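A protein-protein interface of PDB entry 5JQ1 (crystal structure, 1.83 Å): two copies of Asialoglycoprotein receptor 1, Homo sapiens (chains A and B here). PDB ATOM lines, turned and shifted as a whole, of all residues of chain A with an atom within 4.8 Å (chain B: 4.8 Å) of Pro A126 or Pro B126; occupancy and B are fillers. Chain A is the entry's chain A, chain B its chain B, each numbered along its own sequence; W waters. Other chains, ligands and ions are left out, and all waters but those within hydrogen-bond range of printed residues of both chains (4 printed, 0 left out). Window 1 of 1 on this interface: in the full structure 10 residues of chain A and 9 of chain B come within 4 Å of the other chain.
Lys A27 touches Gln B124, but with the chains exchanged Gln A124 does not touch Lys B27 (4.1 Å).
Leu A103 touches Pro B126, and with the chains exchanged Pro A126 touches Leu B103.
Gln A124 touches Pro B126, and with the chains exchanged Pro A126 touches Gln B124.
Pro B126 touches its own counterpart, Pro A126.
Printed residues of chain B within 4 Å of Pro A126: Leu B103 (3.5 Å), Gln B124 (3.5 Å), Arg B125 (3.9996 Å) and Pro B126 (3.8 Å).
Printed residues of chain A within 4 Å of Pro B126: Leu A103 (3.6 Å), Gln A124 (3.8 Å), Arg A125 (3.9 Å) and Pro A126 (3.8 Å).
Of the printed residues of chain B, Lys A27 touches Gln B124.
Printed residues of chain A within 4 Å of Gln B124: Gly A26, Lys A27 and Pro A126.
Printed residues of chain A within 4 Å of Leu B103: Gly A26 (2.8 Å) and Pro A126 (3.5 Å).
Of the printed residues of chain A, Arg B125 touches Pro A126.
Of the printed residues of chain B, Gly A26 touches Leu B103 (2.8 Å) and Gln B124 (3.1 Å).
Tyr A127 touches none of the printed residues of chain B.
The nearest printed residue of chain B that does not touch Pro A126 is Ala B28 (7.4 Å).
The nearest printed residue of chain A that does not touch Pro B126 is Ala A28 (7.5 Å).
The nearest printed residue of chain B that does not touch Gly A26 is Arg B125 (8.7 Å).
Gln B124 touches Lys A27.
Leu A103 touches Pro B126 (CD2 to O, 3.6 Å).
CG of Gln A124 touches CB of Pro B126, 3.8 Å away.
Arg A125 touches Pro B126.
O of Pro A126 touches CD2 of Leu B103 (3.5 Å).
CB of Pro A126 touches OE1 of Gln B124 (3.5 Å).
Pro A126 touches Arg B125 (CD to CA, 3.9996 Å).
Pro A126 touches Pro B126 (CD to CD, 3.8 Å).
The backbone NH (N) of Lys A27 is in hydrogen-bond range of the backbone carbonyl oxygen (O) of Tyr A127 (3.0 Å).
The indole nitrogen of Trp A65 is in hydrogen-bond range of the backbone carbonyl oxygen of Lys A27 (2.8 Å).
O of Arg B125 sits close to NE1 of Trp B65.
The indole nitrogen (NE1) of Trp A65 sits close to the backbone carbonyl oxygen (O) of Arg A125, 3.3 Å away.
O of Leu A103 lies within hydrogen-bond range of N of Gly B26 (2.8 Å).
O of Leu B103 sits at hydrogen-bond distance from N of Gly A26.
The side-chain amide oxygen (OE1) of Gln A124 sits close to the backbone carbonyl oxygen (O) of Gly B26 (3.2 Å).
O of Gly A26 sits at hydrogen-bond distance from NE2 of Gln B124 (3.1 Å).
Of the 10 printed residues of chain B, 5 touch a printed residue of chain A.
Hydrophobic or aromatic side chains of chain B that line the printed part of chain A: Leu B103 and Pro B126.
Of the 10 printed residues of chain A, 6 touch a printed residue of chain B.
Printed residues of chain A that touch a printed residue of chain B: Gly A26, Lys A27, Leu A103, Gln A124, Arg A125 and Pro A126.
Hydrophobic or aromatic side chains of chain A that line the printed part of chain B: Leu A103 and Pro A126.
Among the printed residues, 12 pairs touch across the chains.
Among the printed residues, no Asp or Glu carboxylate lies within 4 Å of a Lys or Arg side-chain nitrogen of the other chain.
Water W2 bridges the backbone carbonyl oxygen (O) of Gln A124 (2.6 Å) and the backbone carbonyl oxygen (O) of Gln B124 (2.7 Å).
Water W1 lies within hydrogen-bond range of O of Pro B126 (2.7 Å) and NH1 of Arg A125 (3.1 Å).
Water W3 bridges the backbone carbonyl oxygen of Pro A126 (2.7 Å) and the guanidinium group of Arg B125 (2.9 Å).
Water W4 bridges N of Ala B28 (2.9 Å) and OE1 of Gln A124 (3.3 Å).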
ATOM      1  N   GLY A  26     -13.591  13.626   6.440  1.00  0.00           N
ATOM      2  CA  GLY A  26     -13.037  13.454   7.784  1.00  0.00           C
ATOM      3  C   GLY A  26     -13.525  12.251   8.566  1.00  0.00           C
ATOM      4  O   GLY A  26     -14.643  11.785   8.372  1.00  0.00           O
ATOM      5  N   LYS A  27     -12.678  11.762   9.485  1.00  0.00           N
ATOM      6  CA  LYS A  27     -12.960  10.667  10.397  1.00  0.00           C
ATOM      7  C   LYS A  27     -12.203  10.896  11.701  1.00  0.00           C
ATOM      8  O   LYS A  27     -11.129  11.533  11.716  1.00  0.00           O
ATOM      9  CB  LYS A  27     -12.523   9.298   9.808  1.00  0.00           C
ATOM     10  CG  LYS A  27     -13.560   8.622   8.910  1.00  0.00           C
ATOM     11  CD  LYS A  27     -13.053   7.276   8.395  1.00  0.00           C
ATOM     12  CE  LYS A  27     -13.899   6.709   7.263  1.00  0.00           C
ATOM     13  NZ  LYS A  27     -15.261   6.312   7.703  1.00  0.00           N
ATOM     14  N   ALA A  28     -12.751  10.333  12.788  1.00  0.00           N
ATOM     15  CA  ALA A  28     -12.106  10.259  14.089  1.00  0.00           C
ATOM     16  C   ALA A  28     -10.840   9.397  13.839  1.00  0.00           C
ATOM     17  O   ALA A  28     -10.850   8.546  12.930  1.00  0.00           O
ATOM     18  CB  ALA A  28     -13.021   9.541  15.074  1.00  0.00           C
ATOM     19  N   TRP A  65      -4.903  13.676   9.981  1.00  0.00           N
ATOM     20  CA  TRP A  65      -4.339  12.646  10.862  1.00  0.00           C
ATOM     21  C   TRP A  65      -3.192  11.895  10.190  1.00  0.00           C
ATOM     22  O   TRP A  65      -3.224  11.662   8.975  1.00  0.00           O
ATOM     23  CB  TRP A  65      -5.399  11.578  11.188  1.00  0.00           C
ATOM     24  CG  TRP A  65      -6.543  12.016  12.055  1.00  0.00           C
ATOM     25  CD1 TRP A  65      -7.874  11.816  11.804  1.00  0.00           C
ATOM     26  CD2 TRP A  65      -6.464  12.583  13.378  1.00  0.00           C
ATOM     27  NE1 TRP A  65      -8.628  12.259  12.870  1.00  0.00           N
ATOM     28  CE2 TRP A  65      -7.791  12.739  13.846  1.00  0.00           C
ATOM     29  CE3 TRP A  65      -5.400  13.023  14.195  1.00  0.00           C
ATOM     30  CZ2 TRP A  65      -8.083  13.273  15.113  1.00  0.00           C
ATOM     31  CZ3 TRP A  65      -5.691  13.578  15.444  1.00  0.00           C
ATOM     32  CH2 TRP A  65      -7.013  13.680  15.898  1.00  0.00           C
ATOM     33  N   LEU A 103     -13.094  18.030  26.706  1.00  0.00           N
ATOM     34  CA  LEU A 103     -13.776  16.883  26.087  1.00  0.00           C
ATOM     35  C   LEU A 103     -13.520  15.542  26.778  1.00  0.00           C
ATOM     36  O   LEU A 103     -14.148  14.541  26.429  1.00  0.00           O
ATOM     37  CB  LEU A 103     -13.450  16.785  24.593  1.00  0.00           C
ATOM     38  CG  LEU A 103     -13.735  18.055  23.762  1.00  0.00           C
ATOM     39  CD1 LEU A 103     -13.231  17.883  22.343  1.00  0.00           C
ATOM     40  CD2 LEU A 103     -15.231  18.452  23.846  1.00  0.00           C
ATOM     41  N   GLN A 124     -10.984  11.695  18.985  1.00  0.00           N
ATOM     42  CA  GLN A 124     -12.343  11.709  18.446  1.00  0.00           C
ATOM     43  C   GLN A 124     -12.611  12.868  17.453  1.00  0.00           C
ATOM     44  O   GLN A 124     -13.647  12.843  16.796  1.00  0.00           O
ATOM     45  CB  GLN A 124     -13.425  11.652  19.562  1.00  0.00           C
ATOM     46  CG  GLN A 124     -13.187  12.509  20.790  1.00  0.00           C
ATOM     47  CD  GLN A 124     -14.161  12.279  21.935  1.00  0.00           C
ATOM     48  OE1 GLN A 124     -15.184  11.591  21.819  1.00  0.00           O
ATOM     49  NE2 GLN A 124     -13.867  12.881  23.077  1.00  0.00           N
ATOM     50  N   ARG A 125     -11.723  13.870  17.311  1.00  0.00           N
ATOM     51  CA  ARG A 125     -12.020  14.923  16.328  1.00  0.00           C
ATOM     52  C   ARG A 125     -12.014  14.404  14.884  1.00  0.00           C
ATOM     53  O   ARG A 125     -11.115  13.664  14.502  1.00  0.00           O
ATOM     54  CB  ARG A 125     -11.001  16.064  16.386  1.00  0.00           C
ATOM     55  CG  ARG A 125     -10.906  16.753  17.713  1.00  0.00           C
ATOM     56  CD  ARG A 125     -10.320  18.131  17.474  1.00  0.00           C
ATOM     57  NE  ARG A 125     -10.052  18.760  18.751  1.00  0.00           N
ATOM     58  CZ  ARG A 125     -10.954  19.438  19.433  1.00  0.00           C
ATOM     59  NH1 ARG A 125     -12.184  19.591  18.951  1.00  0.00           N
ATOM     60  NH2 ARG A 125     -10.639  19.974  20.597  1.00  0.00           N
ATOM     61  N   PRO A 126     -12.973  14.820  14.047  1.00  0.00           N
ATOM     62  CA  PRO A 126     -12.941  14.381  12.641  1.00  0.00           C
ATOM     63  C   PRO A 126     -11.959  15.241  11.856  1.00  0.00           C
ATOM     64  O   PRO A 126     -12.085  16.483  11.833  1.00  0.00           O
ATOM     65  CB  PRO A 126     -14.387  14.602  12.181  1.00  0.00           C
ATOM     66  CG  PRO A 126     -14.898  15.709  13.026  1.00  0.00           C
ATOM     67  CD  PRO A 126     -14.154  15.660  14.340  1.00  0.00           C
ATOM     68  N   TYR A 127     -10.951  14.596  11.243  1.00  0.00           N
ATOM     69  CA  TYR A 127     -10.017  15.279  10.376  1.00  0.00           C
ATOM     70  C   TYR A 127      -9.832  14.399   9.168  1.00  0.00           C
ATOM     71  O   TYR A 127     -10.074  13.179   9.220  1.00  0.00           O
ATOM     72  CB  TYR A 127      -8.610  15.430  11.044  1.00  0.00           C
ATOM     73  CG  TYR A 127      -8.447  16.485  12.113  1.00  0.00           C
ATOM     74  CD1 TYR A 127      -9.145  17.693  12.048  1.00  0.00           C
ATOM     75  CD2 TYR A 127      -7.503  16.330  13.125  1.00  0.00           C
ATOM     76  CE1 TYR A 127      -8.964  18.687  13.016  1.00  0.00           C
ATOM     77  CE2 TYR A 127      -7.334  17.298  14.113  1.00  0.00           C
ATOM     78  CZ  TYR A 127      -8.045  18.487  14.041  1.00  0.00           C
ATOM     79  OH  TYR A 127      -7.791  19.463  14.974  1.00  0.00           O
ATOM     80  N   ARG A 128      -9.330  14.998   8.102  1.00  0.00           N
ATOM     81  CA  ARG A 128      -8.924  14.282   6.904  1.00  0.00           C
ATOM     82  C   ARG A 128      -7.736  13.407   7.338  1.00  0.00           C
ATOM     83  O   ARG A 128      -7.236  13.577   8.452  1.00  0.00           O
ATOM     84  CB  ARG A 128      -8.512  15.268   5.795  1.00  0.00           C
ATOM     85  CG  ARG A 128      -9.724  15.964   5.190  1.00  0.00           C
ATOM     86  CD  ARG A 128      -9.383  16.826   3.996  1.00  0.00           C
ATOM     87  NE  ARG A 128     -10.609  17.311   3.355  1.00  0.00           N
ATOM     88  CZ  ARG A 128     -10.658  17.978   2.202  1.00  0.00           C
ATOM     89  NH1 ARG A 128      -9.537  18.304   1.565  1.00  0.00           N
ATOM     90  NH2 ARG A 128     -11.832  18.335   1.683  1.00  0.00           N
ATOM     91  N   GLY B  26     -16.839  15.178  25.919  1.00  0.00           N
ATOM     92  CA  GLY B  26     -17.442  15.322  24.600  1.00  0.00           C
ATOM     93  C   GLY B  26     -17.683  14.034  23.855  1.00  0.00           C
ATOM     94  O   GLY B  26     -16.974  13.045  24.057  1.00  0.00           O
ATOM     95  N   LYS B  27     -18.663  14.068  22.950  1.00  0.00           N
ATOM     96  CA  LYS B  27     -19.038  12.960  22.086  1.00  0.00           C
ATOM     97  C   LYS B  27     -19.560  13.472  20.758  1.00  0.00           C
ATOM     98  O   LYS B  27     -20.123  14.576  20.692  1.00  0.00           O
ATOM     99  CB  LYS B  27     -20.159  12.118  22.757  1.00  0.00           C
ATOM    100  CG  LYS B  27     -19.661  11.049  23.736  1.00  0.00           C
ATOM    101  CD  LYS B  27     -20.824  10.275  24.374  1.00  0.00           C
ATOM    102  CE  LYS B  27     -20.386   9.345  25.526  1.00  0.00           C
ATOM    103  NZ  LYS B  27     -19.645   8.137  25.043  1.00  0.00           N
ATOM    104  N   ALA B  28     -19.425  12.639  19.703  1.00  0.00           N
ATOM    105  CA  ALA B  28     -20.039  12.885  18.402  1.00  0.00           C
ATOM    106  C   ALA B  28     -21.563  12.808  18.680  1.00  0.00           C
ATOM    107  O   ALA B  28     -21.977  12.097  19.607  1.00  0.00           O
ATOM    108  CB  ALA B  28     -19.609  11.796  17.407  1.00  0.00           C
ATOM    109  N   TRP B  65     -24.121  19.836  22.272  1.00  0.00           N
ATOM    110  CA  TRP B  65     -25.186  19.223  21.448  1.00  0.00           C
ATOM    111  C   TRP B  65     -26.553  19.269  22.113  1.00  0.00           C
ATOM    112  O   TRP B  65     -26.662  19.068  23.324  1.00  0.00           O
ATOM    113  CB  TRP B  65     -24.876  17.746  21.146  1.00  0.00           C
ATOM    114  CG  TRP B  65     -23.704  17.468  20.239  1.00  0.00           C
ATOM    115  CD1 TRP B  65     -22.704  16.581  20.473  1.00  0.00           C
ATOM    116  CD2 TRP B  65     -23.488  17.974  18.901  1.00  0.00           C
ATOM    117  NE1 TRP B  65     -21.844  16.533  19.392  1.00  0.00           N
ATOM    118  CE2 TRP B  65     -22.292  17.390  18.421  1.00  0.00           C
ATOM    119  CE3 TRP B  65     -24.181  18.869  18.067  1.00  0.00           C
ATOM    120  CZ2 TRP B  65     -21.773  17.669  17.143  1.00  0.00           C
ATOM    121  CZ3 TRP B  65     -23.647  19.181  16.824  1.00  0.00           C
ATOM    122  CH2 TRP B  65     -22.473  18.564  16.358  1.00  0.00           C
ATOM    123  N   LEU B 103     -15.086  18.058   5.579  1.00  0.00           N
ATOM    124  CA  LEU B 103     -15.180  16.763   6.282  1.00  0.00           C
ATOM    125  C   LEU B 103     -16.181  15.772   5.669  1.00  0.00           C
ATOM    126  O   LEU B 103     -16.230  14.613   6.084  1.00  0.00           O
ATOM    127  CB  LEU B 103     -15.494  16.957   7.784  1.00  0.00           C
ATOM    128  CG  LEU B 103     -14.541  17.865   8.561  1.00  0.00           C
ATOM    129  CD1 LEU B 103     -15.095  18.157   9.938  1.00  0.00           C
ATOM    130  CD2 LEU B 103     -13.077  17.303   8.577  1.00  0.00           C
ATOM    131  N   GLN B 124     -20.277  14.416  13.478  1.00  0.00           N
ATOM    132  CA  GLN B 124     -19.163  13.673  14.064  1.00  0.00           C
ATOM    133  C   GLN B 124     -18.252  14.547  14.981  1.00  0.00           C
ATOM    134  O   GLN B 124     -17.405  13.978  15.667  1.00  0.00           O
ATOM    135  CB  GLN B 124     -18.370  12.885  12.990  1.00  0.00           C
ATOM    136  CG  GLN B 124     -17.949  13.633  11.769  1.00  0.00           C
ATOM    137  CD  GLN B 124     -17.105  12.795  10.826  1.00  0.00           C
ATOM    138  OE1 GLN B 124     -16.371  11.883  11.229  1.00  0.00           O
ATOM    139  NE2 GLN B 124     -17.117  13.155   9.564  1.00  0.00           N
ATOM    140  N   ARG B 125     -18.456  15.896  15.074  1.00  0.00           N
ATOM    141  CA  ARG B 125     -17.640  16.705  15.999  1.00  0.00           C
ATOM    142  C   ARG B 125     -17.923  16.356  17.466  1.00  0.00           C
ATOM    143  O   ARG B 125     -19.089  16.295  17.870  1.00  0.00           O
ATOM    144  CB  ARG B 125     -17.856  18.228  15.851  1.00  0.00           C
ATOM    145  CG  ARG B 125     -17.417  18.804  14.536  1.00  0.00           C
ATOM    146  CD  ARG B 125     -17.150  20.298  14.680  1.00  0.00           C
ATOM    147  NE  ARG B 125     -17.065  20.926  13.361  1.00  0.00           N
ATOM    148  CZ  ARG B 125     -15.977  20.931  12.599  1.00  0.00           C
ATOM    149  NH1 ARG B 125     -14.846  20.371  13.033  1.00  0.00           N
ATOM    150  NH2 ARG B 125     -16.004  21.499  11.406  1.00  0.00           N
ATOM    151  N   PRO B 126     -16.852  16.141  18.273  1.00  0.00           N
ATOM    152  CA  PRO B 126     -17.069  15.855  19.699  1.00  0.00           C
ATOM    153  C   PRO B 126     -17.405  17.135  20.441  1.00  0.00           C
ATOM    154  O   PRO B 126     -16.602  18.075  20.497  1.00  0.00           O
ATOM    155  CB  PRO B 126     -15.736  15.235  20.152  1.00  0.00           C
ATOM    156  CG  PRO B 126     -14.695  15.843  19.215  1.00  0.00           C
ATOM    157  CD  PRO B 126     -15.418  16.112  17.905  1.00  0.00           C
ATOM    158  N   TYR B 127     -18.597  17.173  21.025  1.00  0.00           N
ATOM    159  CA  TYR B 127     -18.990  18.309  21.838  1.00  0.00           C
ATOM    160  C   TYR B 127     -19.594  17.750  23.111  1.00  0.00           C
ATOM    161  O   TYR B 127     -20.043  16.586  23.139  1.00  0.00           O
ATOM    162  CB  TYR B 127     -20.077  19.157  21.108  1.00  0.00           C
ATOM    163  CG  TYR B 127     -19.633  20.082  19.989  1.00  0.00           C
ATOM    164  CD1 TYR B 127     -18.376  20.701  20.018  1.00  0.00           C
ATOM    165  CD2 TYR B 127     -20.522  20.464  18.985  1.00  0.00           C
ATOM    166  CE1 TYR B 127     -17.997  21.621  19.034  1.00  0.00           C
ATOM    167  CE2 TYR B 127     -20.149  21.369  17.991  1.00  0.00           C
ATOM    168  CZ  TYR B 127     -18.895  21.959  18.028  1.00  0.00           C
ATOM    169  OH  TYR B 127     -18.567  22.851  17.024  1.00  0.00           O
ATOM    170  N   ARG B 128     -19.653  18.581  24.154  1.00  0.00           N
ATOM    171  CA  ARG B 128     -20.381  18.219  25.380  1.00  0.00           C
ATOM    172  C   ARG B 128     -21.871  18.127  24.986  1.00  0.00           C
ATOM    173  O   ARG B 128     -22.246  18.570  23.890  1.00  0.00           O
ATOM    174  CB  ARG B 128     -20.195  19.272  26.479  1.00  0.00           C
ATOM    175  CG  ARG B 128     -18.762  19.300  27.035  1.00  0.00           C
ATOM    176  CD  ARG B 128     -18.622  20.191  28.246  1.00  0.00           C
ATOM    177  NE  ARG B 128     -17.301  20.015  28.857  1.00  0.00           N
ATOM    178  CZ  ARG B 128     -16.934  20.526  30.025  1.00  0.00           C
ATOM    179  NH1 ARG B 128     -17.782  21.261  30.729  1.00  0.00           N
ATOM    180  NH2 ARG B 128     -15.723  20.275  30.517  1.00  0.00           N
HETATM  181  O   HOH W   1     -15.014  20.203  19.977  1.00  0.00           O
HETATM  182  O   HOH W   2     -15.901  11.831  16.076  1.00  0.00           O
HETATM  183  O   HOH W   3     -12.378  19.178  12.137  1.00  0.00           O
HETATM  184  O   HOH W   4     -17.725  10.383  20.096  1.00  0.00           O
